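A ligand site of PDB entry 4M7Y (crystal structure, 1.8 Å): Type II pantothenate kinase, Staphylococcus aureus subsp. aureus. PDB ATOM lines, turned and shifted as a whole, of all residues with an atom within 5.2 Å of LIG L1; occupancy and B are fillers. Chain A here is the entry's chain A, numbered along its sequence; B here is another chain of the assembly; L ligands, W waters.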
ATOM      1  N   ASP A   6      22.088 -35.031 -23.679  1.00  0.00           N
ATOM      2  CA  ASP A   6      23.137 -35.028 -22.689  1.00  0.00           C
ATOM      3  C   ASP A   6      22.442 -35.245 -21.355  1.00  0.00           C
ATOM      4  O   ASP A   6      21.849 -34.337 -20.801  1.00  0.00           O
ATOM      5  CB  ASP A   6      23.865 -33.709 -22.763  1.00  0.00           C
ATOM      6  CG  ASP A   6      24.979 -33.557 -21.754  1.00  0.00           C
ATOM      7  OD1 ASP A   6      25.145 -34.431 -20.880  1.00  0.00           O
ATOM      8  OD2 ASP A   6      25.721 -32.508 -21.842  1.00  0.00           O
ATOM      9  N   ALA A   7      22.497 -36.464 -20.875  1.00  0.00           N
ATOM     10  CA  ALA A   7      21.855 -36.887 -19.637  1.00  0.00           C
ATOM     11  C   ALA A   7      22.897 -36.830 -18.524  1.00  0.00           C
ATOM     12  O   ALA A   7      23.727 -37.716 -18.392  1.00  0.00           O
ATOM     13  CB  ALA A   7      21.310 -38.320 -19.780  1.00  0.00           C
ATOM     14  N   GLY A   8      22.862 -35.752 -17.745  1.00  0.00           N
ATOM     15  CA  GLY A   8      23.876 -35.518 -16.709  1.00  0.00           C
ATOM     16  C   GLY A   8      23.398 -35.917 -15.333  1.00  0.00           C
ATOM     17  O   GLY A   8      22.381 -36.599 -15.184  1.00  0.00           O
ATOM     18  N   GLY A   9      24.134 -35.455 -14.309  1.00  0.00           N
ATOM     19  CA  GLY A   9      23.825 -35.753 -12.938  1.00  0.00           C
ATOM     20  C   GLY A   9      22.594 -35.014 -12.423  1.00  0.00           C
ATOM     21  O   GLY A   9      21.996 -35.470 -11.493  1.00  0.00           O
ATOM     22  N   THR A  10      22.246 -33.865 -13.001  1.00  0.00           N
ATOM     23  CA  THR A  10      21.022 -33.117 -12.550  1.00  0.00           C
ATOM     24  C   THR A  10      19.984 -32.880 -13.646  1.00  0.00           C
ATOM     25  O   THR A  10      18.788 -33.060 -13.418  1.00  0.00           O
ATOM     26  CB  THR A  10      21.415 -31.756 -11.914  1.00  0.00           C
ATOM     27  OG1 THR A  10      22.454 -31.961 -10.971  1.00  0.00           O
ATOM     28  CG2 THR A  10      20.241 -31.101 -11.192  1.00  0.00           C
ATOM     29  N   LEU A  11      20.435 -32.501 -14.837  1.00  0.00           N
ATOM     30  CA  LEU A  11      19.523 -32.211 -15.931  1.00  0.00           C
ATOM     31  C   LEU A  11      19.761 -33.085 -17.157  1.00  0.00           C
ATOM     32  O   LEU A  11      20.893 -33.486 -17.444  1.00  0.00           O
ATOM     33  CB  LEU A  11      19.661 -30.751 -16.347  1.00  0.00           C
ATOM     34  CG  LEU A  11      19.240 -29.714 -15.287  1.00  0.00           C
ATOM     35  CD1 LEU A  11      19.633 -28.325 -15.764  1.00  0.00           C
ATOM     36  CD2 LEU A  11      17.730 -29.782 -15.009  1.00  0.00           C
ATOM     37  N   LYS A  13      19.405 -32.642 -20.988  1.00  0.00           N
ATOM     38  CA  LYS A  13      19.308 -31.665 -22.029  1.00  0.00           C
ATOM     39  C   LYS A  13      18.978 -32.372 -23.335  1.00  0.00           C
ATOM     40  O   LYS A  13      19.693 -33.311 -23.734  1.00  0.00           O
ATOM     41  CB  LYS A  13      20.622 -30.913 -22.183  1.00  0.00           C
ATOM     42  CG  LYS A  13      20.832 -29.794 -21.199  1.00  0.00           C
ATOM     43  CD  LYS A  13      21.217 -30.269 -19.804  1.00  0.00           C
ATOM     44  CE  LYS A  13      22.532 -31.034 -19.788  1.00  0.00           C
ATOM     45  NZ  LYS A  13      22.853 -31.405 -18.386  1.00  0.00           N
ATOM     46  N   LEU A  28      14.471 -32.861 -15.585  1.00  0.00           N
ATOM     47  CA  LEU A  28      15.263 -33.266 -14.449  1.00  0.00           C
ATOM     48  C   LEU A  28      15.695 -34.707 -14.635  1.00  0.00           C
ATOM     49  O   LEU A  28      14.933 -35.524 -15.132  1.00  0.00           O
ATOM     50  CB  LEU A  28      14.454 -33.136 -13.144  1.00  0.00           C
ATOM     51  CG  LEU A  28      14.043 -31.730 -12.685  1.00  0.00           C
ATOM     52  CD1 LEU A  28      13.254 -31.825 -11.385  1.00  0.00           C
ATOM     53  CD2 LEU A  28      15.263 -30.834 -12.496  1.00  0.00           C
ATOM     54  N   THR A  29      16.931 -35.004 -14.225  1.00  0.00           N
ATOM     55  CA  THR A  29      17.468 -36.368 -14.216  1.00  0.00           C
ATOM     56  C   THR A  29      16.615 -37.282 -13.346  1.00  0.00           C
ATOM     57  O   THR A  29      16.468 -38.477 -13.670  1.00  0.00           O
ATOM     58  CB  THR A  29      18.943 -36.349 -13.775  1.00  0.00           C
ATOM     59  OG1 THR A  29      19.720 -35.614 -14.750  1.00  0.00           O
ATOM     60  CG2 THR A  29      19.505 -37.734 -13.630  1.00  0.00           C
ATOM     61  N   ASN A  96      33.187 -26.199 -18.074  1.00  0.00           N
ATOM     62  CA  ASN A  96      31.869 -26.793 -18.057  1.00  0.00           C
ATOM     63  C   ASN A  96      31.374 -26.913 -16.617  1.00  0.00           C
ATOM     64  O   ASN A  96      31.740 -27.841 -15.874  1.00  0.00           O
ATOM     65  CB  ASN A  96      31.906 -28.154 -18.754  1.00  0.00           C
ATOM     66  CG  ASN A  96      30.529 -28.660 -19.131  1.00  0.00           C
ATOM     67  OD1 ASN A  96      29.499 -28.196 -18.613  1.00  0.00           O
ATOM     68  ND2 ASN A  96      30.487 -29.596 -20.065  1.00  0.00           N
ATOM     69  N   VAL A  97      30.551 -25.942 -16.221  1.00  0.00           N
ATOM     70  CA  VAL A  97      30.076 -25.844 -14.843  1.00  0.00           C
ATOM     71  C   VAL A  97      28.690 -26.528 -14.755  1.00  0.00           C
ATOM     72  O   VAL A  97      27.621 -25.860 -14.846  1.00  0.00           O
ATOM     73  CB  VAL A  97      30.021 -24.382 -14.352  1.00  0.00           C
ATOM     74  CG1 VAL A  97      29.783 -24.352 -12.847  1.00  0.00           C
ATOM     75  CG2 VAL A  97      31.315 -23.664 -14.714  1.00  0.00           C
ATOM     76  N   GLY A  98      28.750 -27.858 -14.634  1.00  0.00           N
ATOM     77  CA  GLY A  98      27.561 -28.728 -14.502  1.00  0.00           C
ATOM     78  C   GLY A  98      27.282 -29.080 -13.062  1.00  0.00           C
ATOM     79  O   GLY A  98      27.518 -28.273 -12.167  1.00  0.00           O
ATOM     80  N   THR A  99      26.840 -30.301 -12.791  1.00  0.00           N
ATOM     81  CA  THR A  99      26.678 -30.686 -11.411  1.00  0.00           C
ATOM     82  C   THR A  99      28.029 -30.410 -10.711  1.00  0.00           C
ATOM     83  O   THR A  99      28.070 -29.948  -9.558  1.00  0.00           O
ATOM     84  CB  THR A  99      26.208 -32.130 -11.305  1.00  0.00           C
ATOM     85  OG1 THR A  99      24.927 -32.236 -11.939  1.00  0.00           O
ATOM     86  CG2 THR A  99      26.107 -32.573  -9.848  1.00  0.00           C
ATOM     87  N   GLY A 100      29.108 -30.681 -11.443  1.00  0.00           N
ATOM     88  CA  GLY A 100      30.449 -30.318 -11.029  1.00  0.00           C
ATOM     89  C   GLY A 100      31.166 -29.683 -12.201  1.00  0.00           C
ATOM     90  O   GLY A 100      30.593 -29.527 -13.272  1.00  0.00           O
ATOM     91  N   GLY A 121      27.371 -26.369  -9.881  1.00  0.00           N
ATOM     92  CA  GLY A 121      25.922 -26.367  -9.616  1.00  0.00           C
ATOM     93  C   GLY A 121      25.389 -27.232  -8.512  1.00  0.00           C
ATOM     94  O   GLY A 121      24.432 -26.880  -7.835  1.00  0.00           O
ATOM     95  N   GLY A 122      25.972 -28.420  -8.330  1.00  0.00           N
ATOM     96  CA  GLY A 122      25.563 -29.272  -7.268  1.00  0.00           C
ATOM     97  C   GLY A 122      25.848 -28.745  -5.894  1.00  0.00           C
ATOM     98  O   GLY A 122      25.052 -28.909  -4.992  1.00  0.00           O
ATOM     99  N   ILE A 124      26.127 -25.431  -5.262  1.00  0.00           N
ATOM    100  CA  ILE A 124      25.176 -24.365  -5.116  1.00  0.00           C
ATOM    101  C   ILE A 124      23.837 -24.864  -4.549  1.00  0.00           C
ATOM    102  O   ILE A 124      23.341 -24.338  -3.552  1.00  0.00           O
ATOM    103  CB  ILE A 124      24.980 -23.605  -6.436  1.00  0.00           C
ATOM    104  CG1 ILE A 124      26.284 -22.862  -6.835  1.00  0.00           C
ATOM    105  CG2 ILE A 124      23.813 -22.658  -6.337  1.00  0.00           C
ATOM    106  CD1 ILE A 124      26.255 -22.309  -8.246  1.00  0.00           C
ATOM    107  N   GLN A 125      23.269 -25.889  -5.163  1.00  0.00           N
ATOM    108  CA  GLN A 125      22.030 -26.514  -4.643  1.00  0.00           C
ATOM    109  C   GLN A 125      22.179 -27.132  -3.245  1.00  0.00           C
ATOM    110  O   GLN A 125      21.380 -26.883  -2.392  1.00  0.00           O
ATOM    111  CB  GLN A 125      21.539 -27.563  -5.603  1.00  0.00           C
ATOM    112  CG  GLN A 125      21.018 -26.984  -6.930  1.00  0.00           C
ATOM    113  CD  GLN A 125      20.507 -28.095  -7.822  1.00  0.00           C
ATOM    114  OE1 GLN A 125      21.289 -28.794  -8.480  1.00  0.00           O
ATOM    115  NE2 GLN A 125      19.211 -28.309  -7.789  1.00  0.00           N
ATOM    116  N   TYR A 137      15.170 -24.930  -7.278  1.00  0.00           N
ATOM    117  CA  TYR A 137      16.357 -24.293  -7.855  1.00  0.00           C
ATOM    118  C   TYR A 137      16.135 -22.818  -8.150  1.00  0.00           C
ATOM    119  O   TYR A 137      16.982 -21.985  -7.854  1.00  0.00           O
ATOM    120  CB  TYR A 137      16.798 -24.998  -9.135  1.00  0.00           C
ATOM    121  CG  TYR A 137      17.897 -24.304  -9.815  1.00  0.00           C
ATOM    122  CD1 TYR A 137      19.209 -24.375  -9.322  1.00  0.00           C
ATOM    123  CD2 TYR A 137      17.665 -23.504 -10.953  1.00  0.00           C
ATOM    124  CE1 TYR A 137      20.230 -23.702  -9.935  1.00  0.00           C
ATOM    125  CE2 TYR A 137      18.695 -22.843 -11.585  1.00  0.00           C
ATOM    126  CZ  TYR A 137      19.959 -22.919 -11.073  1.00  0.00           C
ATOM    127  OH  TYR A 137      21.015 -22.271 -11.685  1.00  0.00           O
ATOM    128  N   GLY A 224      27.457 -24.630 -19.200  1.00  0.00           N
ATOM    129  CA  GLY A 224      26.812 -25.423 -18.158  1.00  0.00           C
ATOM    130  C   GLY A 224      25.527 -24.770 -17.668  1.00  0.00           C
ATOM    131  O   GLY A 224      25.379 -23.569 -17.686  1.00  0.00           O
ATOM    132  N   SER A 225      24.605 -25.574 -17.174  1.00  0.00           N
ATOM    133  CA  SER A 225      23.308 -25.060 -16.744  1.00  0.00           C
ATOM    134  C   SER A 225      23.412 -24.314 -15.415  1.00  0.00           C
ATOM    135  O   SER A 225      22.474 -23.645 -15.038  1.00  0.00           O
ATOM    136  CB  SER A 225      22.267 -26.194 -16.616  1.00  0.00           C
ATOM    137  OG  SER A 225      22.296 -27.110 -17.720  1.00  0.00           O
ATOM    138  N   SER A 226      24.558 -24.403 -14.708  1.00  0.00           N
ATOM    139  CA  SER A 226      24.734 -23.669 -13.448  1.00  0.00           C
ATOM    140  C   SER A 226      24.571 -22.171 -13.623  1.00  0.00           C
ATOM    141  O   SER A 226      24.307 -21.520 -12.665  1.00  0.00           O
ATOM    142  CB  SER A 226      26.100 -23.915 -12.841  1.00  0.00           C
ATOM    143  OG  SER A 226      26.270 -25.234 -12.603  1.00  0.00           O
ATOM    144  N   HIS A 228      22.282 -20.794 -15.612  1.00  0.00           N
ATOM    145  CA  HIS A 228      20.859 -20.495 -15.851  1.00  0.00           C
ATOM    146  C   HIS A 228      20.195 -19.930 -14.612  1.00  0.00           C
ATOM    147  O   HIS A 228      20.368 -20.441 -13.530  1.00  0.00           O
ATOM    148  CB  HIS A 228      20.133 -21.755 -16.318  1.00  0.00           C
ATOM    149  CG  HIS A 228      20.576 -22.256 -17.665  1.00  0.00           C
ATOM    150  ND1 HIS A 228      20.109 -23.415 -18.211  1.00  0.00           N
ATOM    151  CD2 HIS A 228      21.468 -21.722 -18.611  1.00  0.00           C
ATOM    152  CE1 HIS A 228      20.665 -23.602 -19.426  1.00  0.00           C
ATOM    153  NE2 HIS A 228      21.484 -22.571 -19.676  1.00  0.00           N
ATOM    154  N   ILE B 159      27.252 -40.017 -10.799  1.00  0.00           N
ATOM    155  CA  ILE B 159      26.795 -39.384 -12.065  1.00  0.00           C
ATOM    156  C   ILE B 159      26.795 -40.412 -13.191  1.00  0.00           C
ATOM    157  O   ILE B 159      25.774 -40.596 -13.865  1.00  0.00           O
ATOM    158  CB  ILE B 159      27.654 -38.133 -12.390  1.00  0.00           C
ATOM    159  CG1 ILE B 159      27.459 -37.096 -11.259  1.00  0.00           C
ATOM    160  CG2 ILE B 159      27.294 -37.514 -13.758  1.00  0.00           C
ATOM    161  CD1 ILE B 159      28.021 -35.710 -11.531  1.00  0.00           C
HETATM  162  P1  LIG L   1      24.560 -32.065 -15.513  1.00  0.00           P
HETATM  163  O1  LIG L   1      25.472 -32.704 -14.517  1.00  0.00           O
HETATM  164  O2  LIG L   1      24.982 -32.416 -16.921  1.00  0.00           O
HETATM  165  O3  LIG L   1      23.116 -32.282 -15.210  1.00  0.00           O
HETATM  166  P2  LIG L   1      24.302 -29.096 -15.958  1.00  0.00           P
HETATM  167  O4  LIG L   1      22.929 -29.267 -16.524  1.00  0.00           O
HETATM  168  O5  LIG L   1      25.367 -28.515 -16.867  1.00  0.00           O
HETATM  169  O6  LIG L   1      24.860 -30.482 -15.244  1.00  0.00           O
HETATM  170  O7  LIG L   1      24.185 -28.246 -14.642  1.00  0.00           O
HETATM  171  C1  LIG L   1      23.371 -28.669 -13.514  1.00  0.00           C
HETATM  172  C2  LIG L   1      23.242 -27.475 -12.592  1.00  0.00           C
HETATM  173  O8  LIG L   1      22.531 -26.405 -13.257  1.00  0.00           O
HETATM  174  C3  LIG L   1      22.504 -27.776 -11.336  1.00  0.00           C
HETATM  175  O9  LIG L   1      23.343 -28.349 -10.303  1.00  0.00           O
HETATM  176  C4  LIG L   1      21.955 -26.443 -10.965  1.00  0.00           C
HETATM  177  O10 LIG L   1      22.904 -25.685 -10.253  1.00  0.00           O
HETATM  178  C5  LIG L   1      21.702 -25.762 -12.321  1.00  0.00           C
HETATM  179  N1  LIG L   1      20.310 -25.751 -12.790  1.00  0.00           N
HETATM  180  C6  LIG L   1      19.884 -24.950 -13.807  1.00  0.00           C
HETATM  181  N2  LIG L   1      18.583 -25.096 -14.047  1.00  0.00           N
HETATM  182  C7  LIG L   1      18.128 -26.005 -13.182  1.00  0.00           C
HETATM  183  C8  LIG L   1      16.850 -26.598 -12.934  1.00  0.00           C
HETATM  184  N3  LIG L   1      15.767 -26.207 -13.685  1.00  0.00           N
HETATM  185  N4  LIG L   1      16.727 -27.515 -11.928  1.00  0.00           N
HETATM  186  C9  LIG L   1      17.785 -27.905 -11.204  1.00  0.00           C
HETATM  187  N5  LIG L   1      19.029 -27.382 -11.411  1.00  0.00           N
HETATM  188  C10 LIG L   1      19.252 -26.457 -12.361  1.00  0.00           C
HETATM  189  O1  LG2 L   2      28.572 -31.801 -16.020  1.00  0.00           O
HETATM  190  P1  LG2 L   2      28.697 -33.015 -15.004  1.00  0.00           P
HETATM  191  O2  LG2 L   2      27.456 -34.037 -15.182  1.00  0.00           O
HETATM  192  O3  LG2 L   2      28.847 -32.624 -13.571  1.00  0.00           O
HETATM  193  O4  LG2 L   2      29.952 -33.866 -15.529  1.00  0.00           O
HETATM  194  C1  LG2 L   2      30.400 -34.933 -14.725  1.00  0.00           C
HETATM  195  C2  LG2 L   2      31.870 -34.719 -14.337  1.00  0.00           C
HETATM  196  C3  LG2 L   2      32.685 -34.695 -15.656  1.00  0.00           C
HETATM  197  C4  LG2 L   2      32.310 -35.888 -13.416  1.00  0.00           C
HETATM  198  C5  LG2 L   2      32.021 -33.314 -13.584  1.00  0.00           C
HETATM  199  O5  LG2 L   2      31.088 -33.276 -12.480  1.00  0.00           O
HETATM  200  C6  LG2 L   2      33.461 -33.101 -13.069  1.00  0.00           C
HETATM  201  O6  LG2 L   2      34.436 -33.109 -13.844  1.00  0.00           O
HETATM  202  N1  LG2 L   2      33.555 -32.885 -11.744  1.00  0.00           N
HETATM  203  C7  LG2 L   2      34.851 -32.626 -11.084  1.00  0.00           C
HETATM  204  C8  LG2 L   2      35.582 -33.970 -10.878  1.00  0.00           C
HETATM  205  C9  LG2 L   2      37.038 -33.679 -10.506  1.00  0.00           C
HETATM  206  O7  LG2 L   2      37.853 -33.379 -11.369  1.00  0.00           O
HETATM  207  N2  LG2 L   2      37.322 -33.696  -9.219  1.00  0.00           N
HETATM  208  C10 LG2 L   2      38.711 -33.387  -8.748  1.00  0.00           C
HETATM  209  C11 LG2 L   2      38.680 -32.824  -7.339  1.00  0.00           C
HETATM  210  C12 LG2 L   2      38.398 -33.962  -6.365  1.00  0.00           C
HETATM  211  C13 LG2 L   2      39.396 -33.988  -5.217  1.00  0.00           C
HETATM  212  C14 LG2 L   2      39.467 -35.395  -4.553  1.00  0.00           C
HETATM  213  O   HOH W   1      27.437 -30.121 -17.784  1.00  0.00           O
HETATM  214  O   HOH W   2      25.244 -28.730 -19.625  1.00  0.00           O
HETATM  215  O   HOH W   3      26.558 -33.988 -18.603  1.00  0.00           O
HETATM  216  O   HOH W   4      18.140 -25.033 -16.956  1.00  0.00           O
HETATM  217  O   HOH W   5      14.404 -28.033 -10.660  1.00  0.00           O
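An oxygen (O1) of LIG L1 lies close to an oxygen (O2) of LG2 L2.
Water W1 lies within hydrogen-bond range of an oxygen (O1) of LG2 L2 (2.7 Å), an oxygen (O5) of LIG L1 (2.8 Å) and the side-chain amide oxygen (OD1) of Asn 96 (2.9 Å). Water W3 lies within hydrogen-bond range of OD1 of Asp 6 and O2 of LIG L1. Water W4 bridges ND1 of His 228 (2.8 Å) and N2 of LIG L1 (2.9 Å).
OE1 of Gln 125 lies within hydrogen-bond range of O9 of LIG L1 (2.8 Å). N of Thr 99 lies within hydrogen-bond range of O6 of LIG L1 (3.2 Å). An oxygen (O3) of LIG L1 sits at hydrogen-bond distance from the backbone NH (N) of Leu 11 (2.7 Å). An oxygen (O1) of LIG L1 is in hydrogen-bond range of the side-chain hydroxyl (OG1) of Thr 99, at 2.7 Å. O of Gly 121 lies close to O9 of LIG L1 (3.1 Å). The side-chain hydroxyl (OG) of Ser 225 sits at hydrogen-bond distance from an oxygen (O4) of LIG L1 (2.5 Å). The backbone NH (N) of Ser 225 lies within hydrogen-bond range of an oxygen (O5) of LIG L1 (3.1 Å). An oxygen (O2) of LIG L1 lies within salt-bridge range of the side-chain amino group (NZ) of Lys 13, at 2.8 Å. An oxygen (O3) of LG2 L2 is in hydrogen-bond range of the backbone NH (N) of Gly 100 (2.9 Å). The backbone NH of Ser 226 sits at hydrogen-bond distance from an oxygen (O8) of LIG L1 (3.2 Å). An oxygen (O3) of LIG L1 is in hydrogen-bond range of the backbone NH (N) of Thr 10 (2.9 Å). N of Gly 9 is in hydrogen-bond range of O1 of LIG L1, at 3.1 Å. The backbone NH (N) of Thr 99 sits at hydrogen-bond distance from an oxygen (O3) of LG2 L2 (3.2 Å). An oxygen (O9) of LIG L1 sits at hydrogen-bond distance from the backbone NH of Gly 122 (3.3 Å).
OG1 of Thr 29 sits at hydrogen-bond distance from O of Gly 8. The backbone carbonyl oxygen (O) of Gly 98 is in hydrogen-bond range of the side-chain hydroxyl (OG) of Ser 226, 3.3 Å away. The side-chain hydroxyl (OH) of Tyr 137 sits at hydrogen-bond distance from the backbone carbonyl oxygen (O) of His 228 (2.7 Å). The backbone NH of Gly 121 is in hydrogen-bond range of the side-chain hydroxyl of Ser 226. The backbone NH (N) of Gly 121 is in hydrogen-bond range of the backbone carbonyl oxygen (O) of Gly 98. O of Thr 10 lies within hydrogen-bond range of N of Thr 29, 2.8 Å away. The backbone carbonyl oxygen (O) of Thr 99 sits at hydrogen-bond distance from the backbone NH (N) of Gly 122, 2.9 Å away. The backbone carbonyl oxygen (O) of Leu 11 lies within hydrogen-bond range of the side-chain amino group (NZ) of Lys 13, at 3.0 Å.
Merely in contact with LIG L1: Gly 8 (3.3 Å), Leu 28 (3.7 Å), Gly 98 (3.2 Å), Tyr 137 (3.3 Å) and Gly 224 (3.6 Å). Of the 24 residues printed, 15 come within 4 Å of LIG L1. The nearest printed residue that does not touch LIG L1 is Val 97 (4.03 Å).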
